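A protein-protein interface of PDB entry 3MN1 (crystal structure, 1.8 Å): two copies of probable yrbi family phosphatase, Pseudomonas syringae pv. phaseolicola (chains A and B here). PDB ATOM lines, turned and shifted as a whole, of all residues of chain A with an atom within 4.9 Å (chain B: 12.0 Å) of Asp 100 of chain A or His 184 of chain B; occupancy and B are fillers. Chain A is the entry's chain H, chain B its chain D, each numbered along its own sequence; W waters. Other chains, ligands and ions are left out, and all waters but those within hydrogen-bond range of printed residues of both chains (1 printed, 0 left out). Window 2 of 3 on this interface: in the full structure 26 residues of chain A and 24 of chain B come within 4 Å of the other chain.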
ATOM      1  N   ASP A  94      -3.944 -13.517   4.997  1.00  0.00           N
ATOM      2  CA  ASP A  94      -4.889 -14.069   5.983  1.00  0.00           C
ATOM      3  C   ASP A  94      -5.992 -14.850   5.280  1.00  0.00           C
ATOM      4  O   ASP A  94      -7.050 -14.335   4.929  1.00  0.00           O
ATOM      5  CB  ASP A  94      -5.463 -13.002   6.930  1.00  0.00           C
ATOM      6  CG  ASP A  94      -6.106 -13.609   8.189  1.00  0.00           C
ATOM      7  OD1 ASP A  94      -6.574 -14.772   8.140  1.00  0.00           O
ATOM      8  OD2 ASP A  94      -6.146 -12.919   9.237  1.00  0.00           O
ATOM      9  N   LEU A  96      -7.902 -17.427   6.378  1.00  0.00           N
ATOM     10  CA  LEU A  96      -9.137 -17.677   7.128  1.00  0.00           C
ATOM     11  C   LEU A  96     -10.108 -16.486   7.038  1.00  0.00           C
ATOM     12  O   LEU A  96     -11.322 -16.661   6.907  1.00  0.00           O
ATOM     13  CB  LEU A  96      -8.828 -18.065   8.572  1.00  0.00           C
ATOM     14  CG  LEU A  96     -10.002 -18.647   9.340  1.00  0.00           C
ATOM     15  CD1 LEU A  96     -10.554 -19.876   8.633  1.00  0.00           C
ATOM     16  CD2 LEU A  96      -9.584 -18.978  10.769  1.00  0.00           C
ATOM     17  N   VAL A  97      -9.571 -15.273   7.063  1.00  0.00           N
ATOM     18  CA  VAL A  97     -10.392 -14.083   6.871  1.00  0.00           C
ATOM     19  C   VAL A  97     -11.098 -14.078   5.525  1.00  0.00           C
ATOM     20  O   VAL A  97     -12.286 -13.762   5.433  1.00  0.00           O
ATOM     21  CB  VAL A  97      -9.566 -12.792   7.053  1.00  0.00           C
ATOM     22  CG1 VAL A  97     -10.317 -11.589   6.516  1.00  0.00           C
ATOM     23  CG2 VAL A  97      -9.198 -12.610   8.531  1.00  0.00           C
ATOM     24  N   VAL A  98     -10.373 -14.457   4.473  1.00  0.00           N
ATOM     25  CA  VAL A  98     -10.958 -14.513   3.145  1.00  0.00           C
ATOM     26  C   VAL A  98     -12.041 -15.584   3.104  1.00  0.00           C
ATOM     27  O   VAL A  98     -13.125 -15.366   2.540  1.00  0.00           O
ATOM     28  CB  VAL A  98      -9.876 -14.851   2.074  1.00  0.00           C
ATOM     29  CG1 VAL A  98     -10.530 -15.181   0.725  1.00  0.00           C
ATOM     30  CG2 VAL A  98      -8.887 -13.701   1.937  1.00  0.00           C
ATOM     31  N   LEU A  99     -11.747 -16.741   3.703  1.00  0.00           N
ATOM     32  CA  LEU A  99     -12.664 -17.866   3.636  1.00  0.00           C
ATOM     33  C   LEU A  99     -13.944 -17.488   4.371  1.00  0.00           C
ATOM     34  O   LEU A  99     -15.050 -17.730   3.882  1.00  0.00           O
ATOM     35  CB  LEU A  99     -12.035 -19.119   4.246  1.00  0.00           C
ATOM     36  CG  LEU A  99     -12.964 -20.334   4.225  1.00  0.00           C
ATOM     37  CD1 LEU A  99     -13.333 -20.746   2.801  1.00  0.00           C
ATOM     38  CD2 LEU A  99     -12.348 -21.508   4.996  1.00  0.00           C
ATOM     39  N   ASP A 100     -13.795 -16.854   5.530  1.00  0.00           N
ATOM     40  CA  ASP A 100     -14.964 -16.496   6.339  1.00  0.00           C
ATOM     41  C   ASP A 100     -15.954 -15.628   5.560  1.00  0.00           C
ATOM     42  O   ASP A 100     -17.173 -15.840   5.627  1.00  0.00           O
ATOM     43  CB  ASP A 100     -14.547 -15.780   7.621  1.00  0.00           C
ATOM     44  CG  ASP A 100     -14.039 -16.724   8.688  1.00  0.00           C
ATOM     45  OD1 ASP A 100     -14.209 -17.958   8.563  1.00  0.00           O
ATOM     46  OD2 ASP A 100     -13.478 -16.221   9.683  1.00  0.00           O
ATOM     47  N   LYS A 101     -15.420 -14.664   4.815  1.00  0.00           N
ATOM     48  CA  LYS A 101     -16.221 -13.728   4.020  1.00  0.00           C
ATOM     49  C   LYS A 101     -16.913 -14.435   2.860  1.00  0.00           C
ATOM     50  O   LYS A 101     -18.109 -14.244   2.605  1.00  0.00           O
ATOM     51  CB  LYS A 101     -15.318 -12.609   3.499  1.00  0.00           C
ATOM     52  CG  LYS A 101     -16.045 -11.481   2.786  1.00  0.00           C
ATOM     53  CD  LYS A 101     -15.090 -10.302   2.572  1.00  0.00           C
ATOM     54  CE  LYS A 101     -15.830  -8.982   2.425  1.00  0.00           C
ATOM     55  NZ  LYS A 101     -16.513  -8.887   1.115  1.00  0.00           N
ATOM     56  N   LEU A 102     -16.161 -15.266   2.149  1.00  0.00           N
ATOM     57  CA  LEU A 102     -16.753 -16.071   1.090  1.00  0.00           C
ATOM     58  C   LEU A 102     -17.866 -16.982   1.615  1.00  0.00           C
ATOM     59  O   LEU A 102     -18.901 -17.136   0.958  1.00  0.00           O
ATOM     60  CB  LEU A 102     -15.662 -16.899   0.391  1.00  0.00           C
ATOM     61  CG  LEU A 102     -16.154 -17.914  -0.633  1.00  0.00           C
ATOM     62  CD1 LEU A 102     -16.925 -17.231  -1.771  1.00  0.00           C
ATOM     63  CD2 LEU A 102     -14.959 -18.716  -1.173  1.00  0.00           C
ATOM     64  N   LEU A 103     -17.655 -17.593   2.784  1.00  0.00           N
ATOM     65  CA  LEU A 103     -18.623 -18.538   3.354  1.00  0.00           C
ATOM     66  C   LEU A 103     -19.946 -17.826   3.693  1.00  0.00           C
ATOM     67  O   LEU A 103     -21.026 -18.405   3.558  1.00  0.00           O
ATOM     68  CB  LEU A 103     -18.053 -19.225   4.597  1.00  0.00           C
ATOM     69  CG  LEU A 103     -16.951 -20.275   4.314  1.00  0.00           C
ATOM     70  CD1 LEU A 103     -16.512 -21.103   5.556  1.00  0.00           C
ATOM     71  CD2 LEU A 103     -17.379 -21.193   3.162  1.00  0.00           C
ATOM     72  N   ALA A 104     -19.836 -16.578   4.132  1.00  0.00           N
ATOM     73  CA  ALA A 104     -21.015 -15.753   4.395  1.00  0.00           C
ATOM     74  C   ALA A 104     -21.778 -15.518   3.096  1.00  0.00           C
ATOM     75  O   ALA A 104     -23.006 -15.577   3.064  1.00  0.00           O
ATOM     76  CB  ALA A 104     -20.613 -14.423   5.031  1.00  0.00           C
ATOM     77  N   TYR A 110     -17.795 -24.149   7.852  1.00  0.00           N
ATOM     78  CA  TYR A 110     -16.517 -24.863   7.714  1.00  0.00           C
ATOM     79  C   TYR A 110     -16.667 -26.340   7.358  1.00  0.00           C
ATOM     80  O   TYR A 110     -15.881 -26.863   6.577  1.00  0.00           O
ATOM     81  CB  TYR A 110     -15.718 -24.774   9.007  1.00  0.00           C
ATOM     82  CG  TYR A 110     -15.190 -23.409   9.334  1.00  0.00           C
ATOM     83  CD1 TYR A 110     -15.135 -22.409   8.372  1.00  0.00           C
ATOM     84  CD2 TYR A 110     -14.735 -23.117  10.622  1.00  0.00           C
ATOM     85  CE1 TYR A 110     -14.614 -21.140   8.688  1.00  0.00           C
ATOM     86  CE2 TYR A 110     -14.213 -21.864  10.940  1.00  0.00           C
ATOM     87  CZ  TYR A 110     -14.164 -20.885   9.971  1.00  0.00           C
ATOM     88  OH  TYR A 110     -13.671 -19.633  10.287  1.00  0.00           O
ATOM     89  N   ALA B 175       7.776 -22.053  18.208  1.00  0.00           N
ATOM     90  CA  ALA B 175       7.082 -20.779  18.185  1.00  0.00           C
ATOM     91  C   ALA B 175       6.705 -20.305  16.785  1.00  0.00           C
ATOM     92  O   ALA B 175       5.628 -19.745  16.584  1.00  0.00           O
ATOM     93  CB  ALA B 175       7.909 -19.708  18.901  1.00  0.00           C
ATOM     94  N   ALA B 176       7.596 -20.500  15.816  1.00  0.00           N
ATOM     95  CA  ALA B 176       7.277 -20.129  14.444  1.00  0.00           C
ATOM     96  C   ALA B 176       6.062 -20.927  13.948  1.00  0.00           C
ATOM     97  O   ALA B 176       5.241 -20.393  13.213  1.00  0.00           O
ATOM     98  CB  ALA B 176       8.474 -20.343  13.516  1.00  0.00           C
ATOM     99  N   HIS B 177       5.967 -22.193  14.341  1.00  0.00           N
ATOM    100  CA  HIS B 177       4.826 -23.026  13.935  1.00  0.00           C
ATOM    101  C   HIS B 177       3.539 -22.639  14.657  1.00  0.00           C
ATOM    102  O   HIS B 177       2.445 -22.750  14.101  1.00  0.00           O
ATOM    103  CB  HIS B 177       5.099 -24.505  14.191  1.00  0.00           C
ATOM    104  CG  HIS B 177       5.994 -25.143  13.182  1.00  0.00           C
ATOM    105  ND1 HIS B 177       6.685 -26.311  13.436  1.00  0.00           N
ATOM    106  CD2 HIS B 177       6.314 -24.782  11.918  1.00  0.00           C
ATOM    107  CE1 HIS B 177       7.384 -26.645  12.367  1.00  0.00           C
ATOM    108  NE2 HIS B 177       7.180 -25.730  11.434  1.00  0.00           N
ATOM    109  N   SER B 178       3.673 -22.195  15.901  1.00  0.00           N
ATOM    110  CA  SER B 178       2.513 -21.889  16.745  1.00  0.00           C
ATOM    111  C   SER B 178       1.595 -20.830  16.156  1.00  0.00           C
ATOM    112  O   SER B 178       0.376 -20.908  16.296  1.00  0.00           O
ATOM    113  CB  SER B 178       2.965 -21.447  18.139  1.00  0.00           C
ATOM    114  OG  SER B 178       3.569 -22.516  18.831  1.00  0.00           O
ATOM    115  N   VAL B 179       2.168 -19.831  15.509  1.00  0.00           N
ATOM    116  CA  VAL B 179       1.348 -18.802  14.914  1.00  0.00           C
ATOM    117  C   VAL B 179       0.276 -19.451  14.033  1.00  0.00           C
ATOM    118  O   VAL B 179      -0.868 -19.021  14.026  1.00  0.00           O
ATOM    119  CB  VAL B 179       2.170 -17.834  14.062  1.00  0.00           C
ATOM    120  CG1 VAL B 179       1.356 -16.574  13.783  1.00  0.00           C
ATOM    121  CG2 VAL B 179       3.472 -17.485  14.766  1.00  0.00           C
ATOM    122  N   TYR B 180       0.648 -20.496  13.305  1.00  0.00           N
ATOM    123  CA  TYR B 180      -0.247 -21.068  12.293  1.00  0.00           C
ATOM    124  C   TYR B 180      -1.266 -22.090  12.825  1.00  0.00           C
ATOM    125  O   TYR B 180      -2.067 -22.637  12.060  1.00  0.00           O
ATOM    126  CB  TYR B 180       0.573 -21.660  11.148  1.00  0.00           C
ATOM    127  CG  TYR B 180       1.415 -20.633  10.431  1.00  0.00           C
ATOM    128  CD1 TYR B 180       0.861 -19.818   9.449  1.00  0.00           C
ATOM    129  CD2 TYR B 180       2.768 -20.483  10.724  1.00  0.00           C
ATOM    130  CE1 TYR B 180       1.623 -18.876   8.784  1.00  0.00           C
ATOM    131  CE2 TYR B 180       3.543 -19.531  10.054  1.00  0.00           C
ATOM    132  CZ  TYR B 180       2.959 -18.733   9.093  1.00  0.00           C
ATOM    133  OH  TYR B 180       3.703 -17.795   8.403  1.00  0.00           O
ATOM    134  N   LEU B 181      -1.245 -22.346  14.127  1.00  0.00           N
ATOM    135  CA  LEU B 181      -2.287 -23.170  14.747  1.00  0.00           C
ATOM    136  C   LEU B 181      -3.521 -22.333  15.095  1.00  0.00           C
ATOM    137  O   LEU B 181      -4.649 -22.844  15.142  1.00  0.00           O
ATOM    138  CB  LEU B 181      -1.751 -23.852  15.998  1.00  0.00           C
ATOM    139  CG  LEU B 181      -0.594 -24.809  15.725  1.00  0.00           C
ATOM    140  CD1 LEU B 181      -0.086 -25.400  17.034  1.00  0.00           C
ATOM    141  CD2 LEU B 181      -1.026 -25.908  14.779  1.00  0.00           C
ATOM    142  N   GLU B 182      -3.307 -21.042  15.333  1.00  0.00           N
ATOM    143  CA  GLU B 182      -4.409 -20.151  15.685  1.00  0.00           C
ATOM    144  C   GLU B 182      -5.140 -19.599  14.450  1.00  0.00           C
ATOM    145  O   GLU B 182      -4.634 -19.666  13.322  1.00  0.00           O
ATOM    146  CB  GLU B 182      -3.916 -19.020  16.592  1.00  0.00           C
ATOM    147  CG  GLU B 182      -2.965 -18.063  15.912  1.00  0.00           C
ATOM    148  CD  GLU B 182      -2.180 -17.213  16.899  1.00  0.00           C
ATOM    149  OE1 GLU B 182      -1.611 -17.777  17.863  1.00  0.00           O
ATOM    150  OE2 GLU B 182      -2.121 -15.982  16.695  1.00  0.00           O
ATOM    151  N   GLY B 183      -6.333 -19.059  14.672  1.00  0.00           N
ATOM    152  CA  GLY B 183      -7.184 -18.580  13.586  1.00  0.00           C
ATOM    153  C   GLY B 183      -6.621 -17.435  12.761  1.00  0.00           C
ATOM    154  O   GLY B 183      -6.196 -17.632  11.616  1.00  0.00           O
ATOM    155  N   HIS B 184      -6.623 -16.232  13.333  1.00  0.00           N
ATOM    156  CA  HIS B 184      -6.244 -15.032  12.590  1.00  0.00           C
ATOM    157  C   HIS B 184      -5.085 -14.287  13.256  1.00  0.00           C
ATOM    158  O   HIS B 184      -4.012 -14.852  13.481  1.00  0.00           O
ATOM    159  CB  HIS B 184      -7.452 -14.100  12.434  1.00  0.00           C
ATOM    160  CG  HIS B 184      -8.741 -14.816  12.155  1.00  0.00           C
ATOM    161  ND1 HIS B 184      -9.411 -15.544  13.114  1.00  0.00           N
ATOM    162  CD2 HIS B 184      -9.488 -14.906  11.028  1.00  0.00           C
ATOM    163  CE1 HIS B 184     -10.510 -16.058  12.589  1.00  0.00           C
ATOM    164  NE2 HIS B 184     -10.582 -15.682  11.325  1.00  0.00           N
HETATM  165  O   HOH W   1     -12.776 -13.715   9.702  1.00  0.00           O
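A ring nitrogen (NE2) of His 184 of chain B lies within hydrogen-bond range of the side-chain carboxylate (OD2) of Asp 100 of chain A, at 3.4 Å.
The side-chain carboxylate (OD1) of Asp 94 of chain A lies close to the backbone NH (N) of Leu 96 of chain A (3.5 Å).
The backbone NH (N) of Val 97 of chain A sits at hydrogen-bond distance from the side-chain carboxylate (OD1) of Asp 94 of chain A.
The side-chain carboxylate of Asp 100 of chain A lies within hydrogen-bond range of the side-chain hydroxyl of Tyr 110 of chain A.
Among the printed residues, pairs that only touch across the chains: Asp 94 of chain A with His 184 of chain B (3.6 Å), Leu 96 of chain A with Gly 183 of chain B (3.7 Å), Leu 96 of chain A with His 184 of chain B (3.5 Å) and Val 97 of chain A with His 184 of chain B (3.4 Å).
Printed residues of chain B within 4 Å of Asp 94 of chain A: His 184.
Of the printed residues of chain B, Leu 96 of chain A touches Gly 183 and His 184.
No residue of chain B comes within 4 Å of Val 98 of chain A.
No residue of chain B comes within 4 Å of Leu 99 of chain A.
Of chain B, only His 184 (3.4 Å) comes within 4 Å of Asp 100 of chain A.
No residue of chain B comes within 4 Å of Ala 104 of chain A.
His 177 of chain B touches none of the printed residues of chain A.
Of the printed residues of chain A, Gly 183 of chain B touches Leu 96.
Printed residues of chain A within 4 Å of His 184 of chain B: Asp 94 (3.6 Å), Leu 96 (3.5 Å), Val 97 (3.4 Å) and Asp 100 (3.4 Å).
The nearest printed residue of chain A that does not touch His 184 of chain B is Tyr 110 of chain A (5.1 Å).
Of the 11 printed residues of chain A, 4 touch a printed residue of chain B.
Hydrophobic or aromatic side chains of chain A within 4 Å of the printed part of chain B: Leu 96 and Val 97.
Along chain A the printed residues that touch a printed residue of chain B span positions 94 to 100.
Among the printed residues, no Asp or Glu carboxylate lies within 4 Å of a Lys or Arg side-chain nitrogen of the other chain.
No position is printed for both chains.
Of the 5 pairs that touch across the chains among the printed residues, none has its exchanged pair printed and touching as well.
Water W1 lies within hydrogen-bond range of the side-chain carboxylate (OD2) of Asp 100 of chain A and a ring nitrogen (NE2) of His 184 of chain B.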
